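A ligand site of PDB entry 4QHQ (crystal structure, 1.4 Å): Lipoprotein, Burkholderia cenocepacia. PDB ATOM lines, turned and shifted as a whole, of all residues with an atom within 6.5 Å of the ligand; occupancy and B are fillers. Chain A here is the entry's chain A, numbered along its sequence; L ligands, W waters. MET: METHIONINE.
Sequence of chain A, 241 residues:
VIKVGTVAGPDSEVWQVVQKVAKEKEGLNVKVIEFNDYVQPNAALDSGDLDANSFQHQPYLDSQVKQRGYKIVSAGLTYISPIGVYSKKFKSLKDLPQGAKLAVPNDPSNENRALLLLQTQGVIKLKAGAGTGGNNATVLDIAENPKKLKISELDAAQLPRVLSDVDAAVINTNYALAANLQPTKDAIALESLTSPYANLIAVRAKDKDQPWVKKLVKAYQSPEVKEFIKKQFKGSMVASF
Water W4 lies within hydrogen-bond range of O of Tyr 197 (2.8 Å), O of the ligand (2.8 Å), N of Ser 81 (2.9 Å) and NH2 of Arg 113 (3.1 Å).
Water W2 lies within hydrogen-bond range of the side-chain hydroxyl of Ser 81, a nitrogen (N) of the ligand and the backbone NH of Asn 174.
Water W1 lies within hydrogen-bond range of OD2 of Asp 11, O of Phe 55 and N of the ligand.
Water W3 lies within hydrogen-bond range of the backbone carbonyl oxygen of Ser 81 (2.8 Å), the backbone NH of Thr 173 (2.9 Å) and an oxygen (OXT) of the ligand (2.9 Å).
Tyr 38 touches the ligand.
Phe 55 touches the ligand (O to CB, 3.3 Å).
CA of Gln 56 touches CE of the ligand (3.7 Å).
CB of Tyr 60 touches SD of the ligand (3.5 Å).
Tyr 79 touches the ligand (OH to N, 3.5 Å).
OD1 of Asn 174 touches CA of the ligand, at 3.5 Å.
Of the 22 residues printed, 12 come within 4 Å of the ligand.
The side-chain amide oxygen (OD1) of Asn 199 is in hydrogen-bond range of a nitrogen (N) of the ligand, 2.8 Å away.
NH1 of Arg 113 is in salt-bridge range of OXT of the ligand (2.8 Å).
OXT of the ligand lies close to OD1 of Asn 172, at 2.9 Å.
The side-chain hydroxyl (OG) of Ser 81 is in hydrogen-bond range of an oxygen (O) of the ligand (3.2 Å).
N of His 57 lies close to SD of the ligand (3.7 Å).
A sulfur (SD) of the ligand lies close to a ring nitrogen (NE2) of His 57, at 3.3 Å.
The side-chain amide nitrogen of Asn 110 lies close to a sulfur (SD) of the ligand, at 3.5 Å.
The guanidinium group (NH2) of Arg 113 lies within hydrogen-bond range of the backbone carbonyl oxygen (O) of Ser 81, 3.2 Å away.
NH1 of Arg 113 lies within hydrogen-bond range of OD1 of Asn 110, at 3.4 Å.
The side-chain amide oxygen of Asn 110 sits close to the side-chain amide oxygen of Asn 172.
NE2 of His 57 is in hydrogen-bond range of OD1 of Asn 110, at 2.9 Å.
The backbone NH (N) of Tyr 60 is in hydrogen-bond range of a ring nitrogen (ND1) of His 57 (3.1 Å).
OD2 of Asp 107 sits at hydrogen-bond distance from ND2 of Asn 110, 2.9 Å away.
The backbone NH (N) of Tyr 60 sits close to the side-chain hydroxyl (OG) of Ser 109 (3.4 Å).
N of Leu 61 lies close to OE1 of Gln 56 (3.5 Å).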
ATOM      1  N   ASP A  11      -7.342 -12.860  -5.471  1.00  0.00           N
ATOM      2  CA  ASP A  11      -6.379 -12.567  -6.528  1.00  0.00           C
ATOM      3  C   ASP A  11      -5.714 -11.205  -6.307  1.00  0.00           C
ATOM      4  O   ASP A  11      -4.490 -11.078  -6.478  1.00  0.00           O
ATOM      5  CB  ASP A  11      -7.028 -12.567  -7.914  1.00  0.00           C
ATOM      6  CG  ASP A  11      -7.460 -13.951  -8.345  1.00  0.00           C
ATOM      7  OD1 ASP A  11      -6.584 -14.818  -8.557  1.00  0.00           O
ATOM      8  OD2 ASP A  11      -8.685 -14.171  -8.475  1.00  0.00           O
ATOM      9  N   TYR A  38     -15.564 -11.669 -13.887  1.00  0.00           N
ATOM     10  CA  TYR A  38     -14.719 -12.346 -14.870  1.00  0.00           C
ATOM     11  C   TYR A  38     -14.842 -11.749 -16.251  1.00  0.00           C
ATOM     12  O   TYR A  38     -14.072 -12.095 -17.139  1.00  0.00           O
ATOM     13  CB  TYR A  38     -15.115 -13.819 -15.004  1.00  0.00           C
ATOM     14  CG  TYR A  38     -14.954 -14.702 -13.791  1.00  0.00           C
ATOM     15  CD1 TYR A  38     -14.027 -14.416 -12.801  1.00  0.00           C
ATOM     16  CD2 TYR A  38     -15.737 -15.849 -13.652  1.00  0.00           C
ATOM     17  CE1 TYR A  38     -13.871 -15.257 -11.695  1.00  0.00           C
ATOM     18  CE2 TYR A  38     -15.596 -16.675 -12.558  1.00  0.00           C
ATOM     19  CZ  TYR A  38     -14.665 -16.380 -11.595  1.00  0.00           C
ATOM     20  OH  TYR A  38     -14.554 -17.230 -10.526  1.00  0.00           O
ATOM     21  N   PHE A  55      -6.553 -14.100 -13.583  1.00  0.00           N
ATOM     22  CA  PHE A  55      -7.859 -14.331 -12.976  1.00  0.00           C
ATOM     23  C   PHE A  55      -8.549 -15.610 -13.451  1.00  0.00           C
ATOM     24  O   PHE A  55      -9.591 -15.942 -12.918  1.00  0.00           O
ATOM     25  CB  PHE A  55      -8.797 -13.154 -13.266  1.00  0.00           C
ATOM     26  CG  PHE A  55      -9.364 -13.192 -14.654  1.00  0.00           C
ATOM     27  CD1 PHE A  55      -8.585 -12.865 -15.751  1.00  0.00           C
ATOM     28  CD2 PHE A  55     -10.690 -13.557 -14.860  1.00  0.00           C
ATOM     29  CE1 PHE A  55      -9.099 -12.908 -17.030  1.00  0.00           C
ATOM     30  CE2 PHE A  55     -11.224 -13.613 -16.138  1.00  0.00           C
ATOM     31  CZ  PHE A  55     -10.426 -13.277 -17.223  1.00  0.00           C
ATOM     32  N   GLN A  56      -8.002 -16.300 -14.449  1.00  0.00           N
ATOM     33  CA  GLN A  56      -8.763 -17.356 -15.103  1.00  0.00           C
ATOM     34  C   GLN A  56      -8.001 -18.659 -15.233  1.00  0.00           C
ATOM     35  O   GLN A  56      -6.781 -18.703 -15.085  1.00  0.00           O
ATOM     36  CB  GLN A  56      -9.161 -16.900 -16.513  1.00  0.00           C
ATOM     37  CG  GLN A  56      -8.025 -16.950 -17.524  1.00  0.00           C
ATOM     38  CD  GLN A  56      -8.273 -16.057 -18.722  1.00  0.00           C
ATOM     39  OE1 GLN A  56      -9.286 -16.198 -19.412  1.00  0.00           O
ATOM     40  NE2 GLN A  56      -7.345 -15.132 -18.968  1.00  0.00           N
ATOM     41  N   HIS A  57      -8.731 -19.730 -15.518  1.00  0.00           N
ATOM     42  CA  HIS A  57      -8.124 -21.003 -15.902  1.00  0.00           C
ATOM     43  C   HIS A  57      -8.149 -21.187 -17.418  1.00  0.00           C
ATOM     44  O   HIS A  57      -8.749 -20.391 -18.136  1.00  0.00           O
ATOM     45  CB  HIS A  57      -8.769 -22.178 -15.140  1.00  0.00           C
ATOM     46  CG  HIS A  57     -10.268 -22.172 -15.154  1.00  0.00           C
ATOM     47  ND1 HIS A  57     -11.007 -22.262 -16.324  1.00  0.00           N
ATOM     48  CD2 HIS A  57     -11.170 -22.132 -14.141  1.00  0.00           C
ATOM     49  CE1 HIS A  57     -12.291 -22.259 -16.025  1.00  0.00           C
ATOM     50  NE2 HIS A  57     -12.420 -22.193 -14.702  1.00  0.00           N
ATOM     51  N   TYR A  60     -11.558 -21.494 -19.238  1.00  0.00           N
ATOM     52  CA  TYR A  60     -12.210 -20.191 -19.384  1.00  0.00           C
ATOM     53  C   TYR A  60     -11.590 -19.386 -20.553  1.00  0.00           C
ATOM     54  O   TYR A  60     -12.324 -18.820 -21.368  1.00  0.00           O
ATOM     55  CB  TYR A  60     -12.130 -19.390 -18.082  1.00  0.00           C
ATOM     56  CG  TYR A  60     -12.955 -18.125 -18.118  1.00  0.00           C
ATOM     57  CD1 TYR A  60     -12.410 -16.922 -18.550  1.00  0.00           C
ATOM     58  CD2 TYR A  60     -14.262 -18.135 -17.692  1.00  0.00           C
ATOM     59  CE1 TYR A  60     -13.180 -15.757 -18.564  1.00  0.00           C
ATOM     60  CE2 TYR A  60     -15.055 -16.987 -17.715  1.00  0.00           C
ATOM     61  CZ  TYR A  60     -14.496 -15.799 -18.157  1.00  0.00           C
ATOM     62  OH  TYR A  60     -15.277 -14.670 -18.176  1.00  0.00           O
ATOM     63  N   LEU A  61     -10.263 -19.334 -20.616  1.00  0.00           N
ATOM     64  CA  LEU A  61      -9.591 -18.625 -21.696  1.00  0.00           C
ATOM     65  C   LEU A  61      -9.983 -19.222 -23.041  1.00  0.00           C
ATOM     66  O   LEU A  61     -10.241 -18.497 -24.008  1.00  0.00           O
ATOM     67  CB  LEU A  61      -8.077 -18.684 -21.496  1.00  0.00           C
ATOM     68  CG  LEU A  61      -7.212 -17.995 -22.545  1.00  0.00           C
ATOM     69  CD1 LEU A  61      -7.678 -16.569 -22.738  1.00  0.00           C
ATOM     70  CD2 LEU A  61      -5.769 -18.047 -22.084  1.00  0.00           C
ATOM     71  N   TYR A  79      -2.200 -20.589  -9.406  1.00  0.00           N
ATOM     72  CA  TYR A  79      -2.676 -21.504  -8.379  1.00  0.00           C
ATOM     73  C   TYR A  79      -3.893 -22.229  -8.907  1.00  0.00           C
ATOM     74  O   TYR A  79      -4.510 -21.793  -9.880  1.00  0.00           O
ATOM     75  CB  TYR A  79      -3.071 -20.745  -7.099  1.00  0.00           C
ATOM     76  CG  TYR A  79      -4.231 -19.822  -7.310  1.00  0.00           C
ATOM     77  CD1 TYR A  79      -5.542 -20.257  -7.186  1.00  0.00           C
ATOM     78  CD2 TYR A  79      -4.011 -18.487  -7.636  1.00  0.00           C
ATOM     79  CE1 TYR A  79      -6.602 -19.399  -7.405  1.00  0.00           C
ATOM     80  CE2 TYR A  79      -5.065 -17.622  -7.838  1.00  0.00           C
ATOM     81  CZ  TYR A  79      -6.363 -18.093  -7.716  1.00  0.00           C
ATOM     82  OH  TYR A  79      -7.417 -17.228  -7.917  1.00  0.00           O
ATOM     83  N   ILE A  80      -4.245 -23.332  -8.232  1.00  0.00           N
ATOM     84  CA  ILE A  80      -5.481 -24.047  -8.485  1.00  0.00           C
ATOM     85  C   ILE A  80      -6.351 -23.967  -7.227  1.00  0.00           C
ATOM     86  O   ILE A  80      -5.837 -23.924  -6.096  1.00  0.00           O
ATOM     87  CB  ILE A  80      -5.207 -25.509  -8.903  1.00  0.00           C
ATOM     88  CG1 ILE A  80      -6.477 -26.209  -9.400  1.00  0.00           C
ATOM     89  CG2 ILE A  80      -4.537 -26.302  -7.768  1.00  0.00           C
ATOM     90  CD1 ILE A  80      -6.191 -27.482 -10.183  1.00  0.00           C
ATOM     91  N   SER A  81      -7.660 -23.909  -7.419  1.00  0.00           N
ATOM     92  CA  SER A  81      -8.560 -23.732  -6.292  1.00  0.00           C
ATOM     93  C   SER A  81      -9.816 -24.551  -6.519  1.00  0.00           C
ATOM     94  O   SER A  81     -10.766 -24.062  -7.137  1.00  0.00           O
ATOM     95  CB  SER A  81      -8.904 -22.258  -6.094  1.00  0.00           C
ATOM     96  OG  SER A  81      -9.491 -21.718  -7.256  1.00  0.00           O
ATOM     97  N   PRO A  82      -9.829 -25.792  -6.030  1.00  0.00           N
ATOM     98  CA  PRO A  82     -10.968 -26.697  -6.195  1.00  0.00           C
ATOM     99  C   PRO A  82     -12.301 -26.029  -5.855  1.00  0.00           C
ATOM    100  O   PRO A  82     -12.451 -25.417  -4.805  1.00  0.00           O
ATOM    101  CB  PRO A  82     -10.653 -27.828  -5.207  1.00  0.00           C
ATOM    102  CG  PRO A  82      -9.164 -27.882  -5.215  1.00  0.00           C
ATOM    103  CD  PRO A  82      -8.744 -26.424  -5.253  1.00  0.00           C
ATOM    104  N   ILE A  83     -13.247 -26.151  -6.770  1.00  0.00           N
ATOM    105  CA  ILE A  83     -14.524 -25.487  -6.596  1.00  0.00           C
ATOM    106  C   ILE A  83     -15.382 -26.285  -5.608  1.00  0.00           C
ATOM    107  O   ILE A  83     -15.357 -27.522  -5.588  1.00  0.00           O
ATOM    108  CB  ILE A  83     -15.227 -25.263  -7.952  1.00  0.00           C
ATOM    109  CG1 ILE A  83     -16.348 -24.228  -7.837  1.00  0.00           C
ATOM    110  CG2 ILE A  83     -15.681 -26.547  -8.586  1.00  0.00           C
ATOM    111  CD1 ILE A  83     -16.779 -23.647  -9.184  1.00  0.00           C
ATOM    112  N   ASP A 107     -21.421 -19.118 -17.078  1.00  0.00           N
ATOM    113  CA  ASP A 107     -20.469 -19.001 -18.172  1.00  0.00           C
ATOM    114  C   ASP A 107     -20.090 -20.415 -18.578  1.00  0.00           C
ATOM    115  O   ASP A 107     -20.111 -21.329 -17.743  1.00  0.00           O
ATOM    116  CB  ASP A 107     -19.236 -18.204 -17.747  1.00  0.00           C
ATOM    117  CG  ASP A 107     -18.491 -18.865 -16.625  1.00  0.00           C
ATOM    118  OD1 ASP A 107     -18.966 -18.775 -15.474  1.00  0.00           O
ATOM    119  OD2 ASP A 107     -17.447 -19.507 -16.885  1.00  0.00           O
ATOM    120  N   SER A 109     -17.506 -22.466 -19.356  1.00  0.00           N
ATOM    121  CA  SER A 109     -16.550 -23.366 -18.731  1.00  0.00           C
ATOM    122  C   SER A 109     -16.827 -23.616 -17.250  1.00  0.00           C
ATOM    123  O   SER A 109     -16.674 -24.731 -16.780  1.00  0.00           O
ATOM    124  CB  SER A 109     -15.102 -22.895 -18.940  1.00  0.00           C
ATOM    125  OG  SER A 109     -14.816 -21.754 -18.167  1.00  0.00           O
ATOM    126  N   ASN A 110     -17.195 -22.590 -16.496  1.00  0.00           N
ATOM    127  CA  ASN A 110     -17.485 -22.850 -15.086  1.00  0.00           C
ATOM    128  C   ASN A 110     -18.849 -23.508 -14.841  1.00  0.00           C
ATOM    129  O   ASN A 110     -18.995 -24.245 -13.865  1.00  0.00           O
ATOM    130  CB  ASN A 110     -17.317 -21.586 -14.254  1.00  0.00           C
ATOM    131  CG  ASN A 110     -15.863 -21.180 -14.154  1.00  0.00           C
ATOM    132  OD1 ASN A 110     -15.055 -21.869 -13.507  1.00  0.00           O
ATOM    133  ND2 ASN A 110     -15.523 -20.079 -14.802  1.00  0.00           N
ATOM    134  N   ARG A 113     -17.972 -27.034 -15.466  1.00  0.00           N
ATOM    135  CA  ARG A 113     -17.224 -27.476 -14.309  1.00  0.00           C
ATOM    136  C   ARG A 113     -18.131 -27.824 -13.136  1.00  0.00           C
ATOM    137  O   ARG A 113     -17.972 -28.862 -12.472  1.00  0.00           O
ATOM    138  CB  ARG A 113     -16.283 -26.353 -13.904  1.00  0.00           C
ATOM    139  CG  ARG A 113     -15.446 -26.632 -12.674  1.00  0.00           C
ATOM    140  CD  ARG A 113     -14.620 -25.399 -12.376  1.00  0.00           C
ATOM    141  NE  ARG A 113     -13.609 -25.644 -11.368  1.00  0.00           N
ATOM    142  CZ  ARG A 113     -12.789 -24.713 -10.899  1.00  0.00           C
ATOM    143  NH1 ARG A 113     -12.908 -23.458 -11.347  1.00  0.00           N
ATOM    144  NH2 ARG A 113     -11.868 -25.024 -10.003  1.00  0.00           N
ATOM    145  N   ASN A 172     -17.324 -20.532  -7.315  1.00  0.00           N
ATOM    146  CA  ASN A 172     -15.884 -20.346  -7.519  1.00  0.00           C
ATOM    147  C   ASN A 172     -15.190 -19.844  -6.263  1.00  0.00           C
ATOM    148  O   ASN A 172     -15.691 -18.978  -5.557  1.00  0.00           O
ATOM    149  CB  ASN A 172     -15.600 -19.378  -8.671  1.00  0.00           C
ATOM    150  CG  ASN A 172     -16.012 -19.934 -10.014  1.00  0.00           C
ATOM    151  OD1 ASN A 172     -15.212 -20.584 -10.720  1.00  0.00           O
ATOM    152  ND2 ASN A 172     -17.252 -19.675 -10.392  1.00  0.00           N
ATOM    153  N   THR A 173     -14.025 -20.404  -5.997  1.00  0.00           N
ATOM    154  CA  THR A 173     -13.329 -20.134  -4.750  1.00  0.00           C
ATOM    155  C   THR A 173     -13.011 -18.644  -4.516  1.00  0.00           C
ATOM    156  O   THR A 173     -13.135 -18.165  -3.397  1.00  0.00           O
ATOM    157  CB  THR A 173     -12.102 -21.039  -4.614  1.00  0.00           C
ATOM    158  OG1 THR A 173     -12.568 -22.375  -4.361  1.00  0.00           O
ATOM    159  CG2 THR A 173     -11.190 -20.590  -3.505  1.00  0.00           C
ATOM    160  N   ASN A 174     -12.659 -17.895  -5.569  1.00  0.00           N
ATOM    161  CA  ASN A 174     -12.361 -16.468  -5.370  1.00  0.00           C
ATOM    162  C   ASN A 174     -13.578 -15.725  -4.796  1.00  0.00           C
ATOM    163  O   ASN A 174     -13.433 -14.904  -3.888  1.00  0.00           O
ATOM    164  CB  ASN A 174     -11.842 -15.804  -6.651  1.00  0.00           C
ATOM    165  CG  ASN A 174     -12.857 -15.790  -7.756  1.00  0.00           C
ATOM    166  OD1 ASN A 174     -13.127 -16.815  -8.389  1.00  0.00           O
ATOM    167  ND2 ASN A 174     -13.456 -14.632  -7.998  1.00  0.00           N
ATOM    168  N   TYR A 197      -8.261 -27.057 -13.971  1.00  0.00           N
ATOM    169  CA  TYR A 197      -8.607 -25.669 -13.680  1.00  0.00           C
ATOM    170  C   TYR A 197      -7.540 -24.809 -12.996  1.00  0.00           C
ATOM    171  O   TYR A 197      -7.866 -23.819 -12.322  1.00  0.00           O
ATOM    172  CB  TYR A 197      -9.953 -25.617 -12.914  1.00  0.00           C
ATOM    173  CG  TYR A 197     -11.036 -26.288 -13.715  1.00  0.00           C
ATOM    174  CD1 TYR A 197     -11.561 -25.693 -14.854  1.00  0.00           C
ATOM    175  CD2 TYR A 197     -11.550 -27.529 -13.336  1.00  0.00           C
ATOM    176  CE1 TYR A 197     -12.534 -26.312 -15.612  1.00  0.00           C
ATOM    177  CE2 TYR A 197     -12.528 -28.156 -14.090  1.00  0.00           C
ATOM    178  CZ  TYR A 197     -13.026 -27.540 -15.212  1.00  0.00           C
ATOM    179  OH  TYR A 197     -14.000 -28.143 -15.966  1.00  0.00           O
ATOM    180  N   ALA A 198      -6.270 -25.136 -13.191  1.00  0.00           N
ATOM    181  CA  ALA A 198      -5.223 -24.247 -12.693  1.00  0.00           C
ATOM    182  C   ALA A 198      -5.388 -22.877 -13.320  1.00  0.00           C
ATOM    183  O   ALA A 198      -5.650 -22.750 -14.506  1.00  0.00           O
ATOM    184  CB  ALA A 198      -3.826 -24.785 -13.017  1.00  0.00           C
ATOM    185  N   ASN A 199      -5.200 -21.852 -12.511  1.00  0.00           N
ATOM    186  CA  ASN A 199      -5.303 -20.496 -12.994  1.00  0.00           C
ATOM    187  C   ASN A 199      -3.979 -20.070 -13.630  1.00  0.00           C
ATOM    188  O   ASN A 199      -2.961 -20.747 -13.481  1.00  0.00           O
ATOM    189  CB  ASN A 199      -5.687 -19.540 -11.855  1.00  0.00           C
ATOM    190  CG  ASN A 199      -7.163 -19.618 -11.490  1.00  0.00           C
ATOM    191  OD1 ASN A 199      -7.738 -18.628 -11.082  1.00  0.00           O
ATOM    192  ND2 ASN A 199      -7.776 -20.804 -11.610  1.00  0.00           N
HETATM  193  N   MET L   1     -10.216 -18.255  -9.826  1.00  0.00           N
HETATM  194  CA  MET L   1     -11.341 -18.895 -10.511  1.00  0.00           C
HETATM  195  C   MET L   1     -11.340 -20.394 -10.274  1.00  0.00           C
HETATM  196  O   MET L   1     -10.275 -20.999 -10.285  1.00  0.00           O
HETATM  197  CB  MET L   1     -11.259 -18.592 -12.014  1.00  0.00           C
HETATM  198  CG  MET L   1     -12.423 -19.184 -12.831  1.00  0.00           C
HETATM  199  SD  MET L   1     -12.240 -18.860 -14.605  1.00  0.00           S
HETATM  200  CE  MET L   1     -12.457 -17.074 -14.657  1.00  0.00           C
HETATM  201  OXT MET L   1     -12.396 -21.003 -10.032  1.00  0.00           O
HETATM  202  O   HOH W   1     -10.361 -15.445 -10.231  1.00  0.00           O
HETATM  203  O   HOH W   2     -10.570 -19.175  -7.215  1.00  0.00           O
HETATM  204  O   HOH W   3     -13.075 -22.510  -7.681  1.00  0.00           O
HETATM  205  O   HOH W   4      -9.195 -23.536  -9.909  1.00  0.00           O
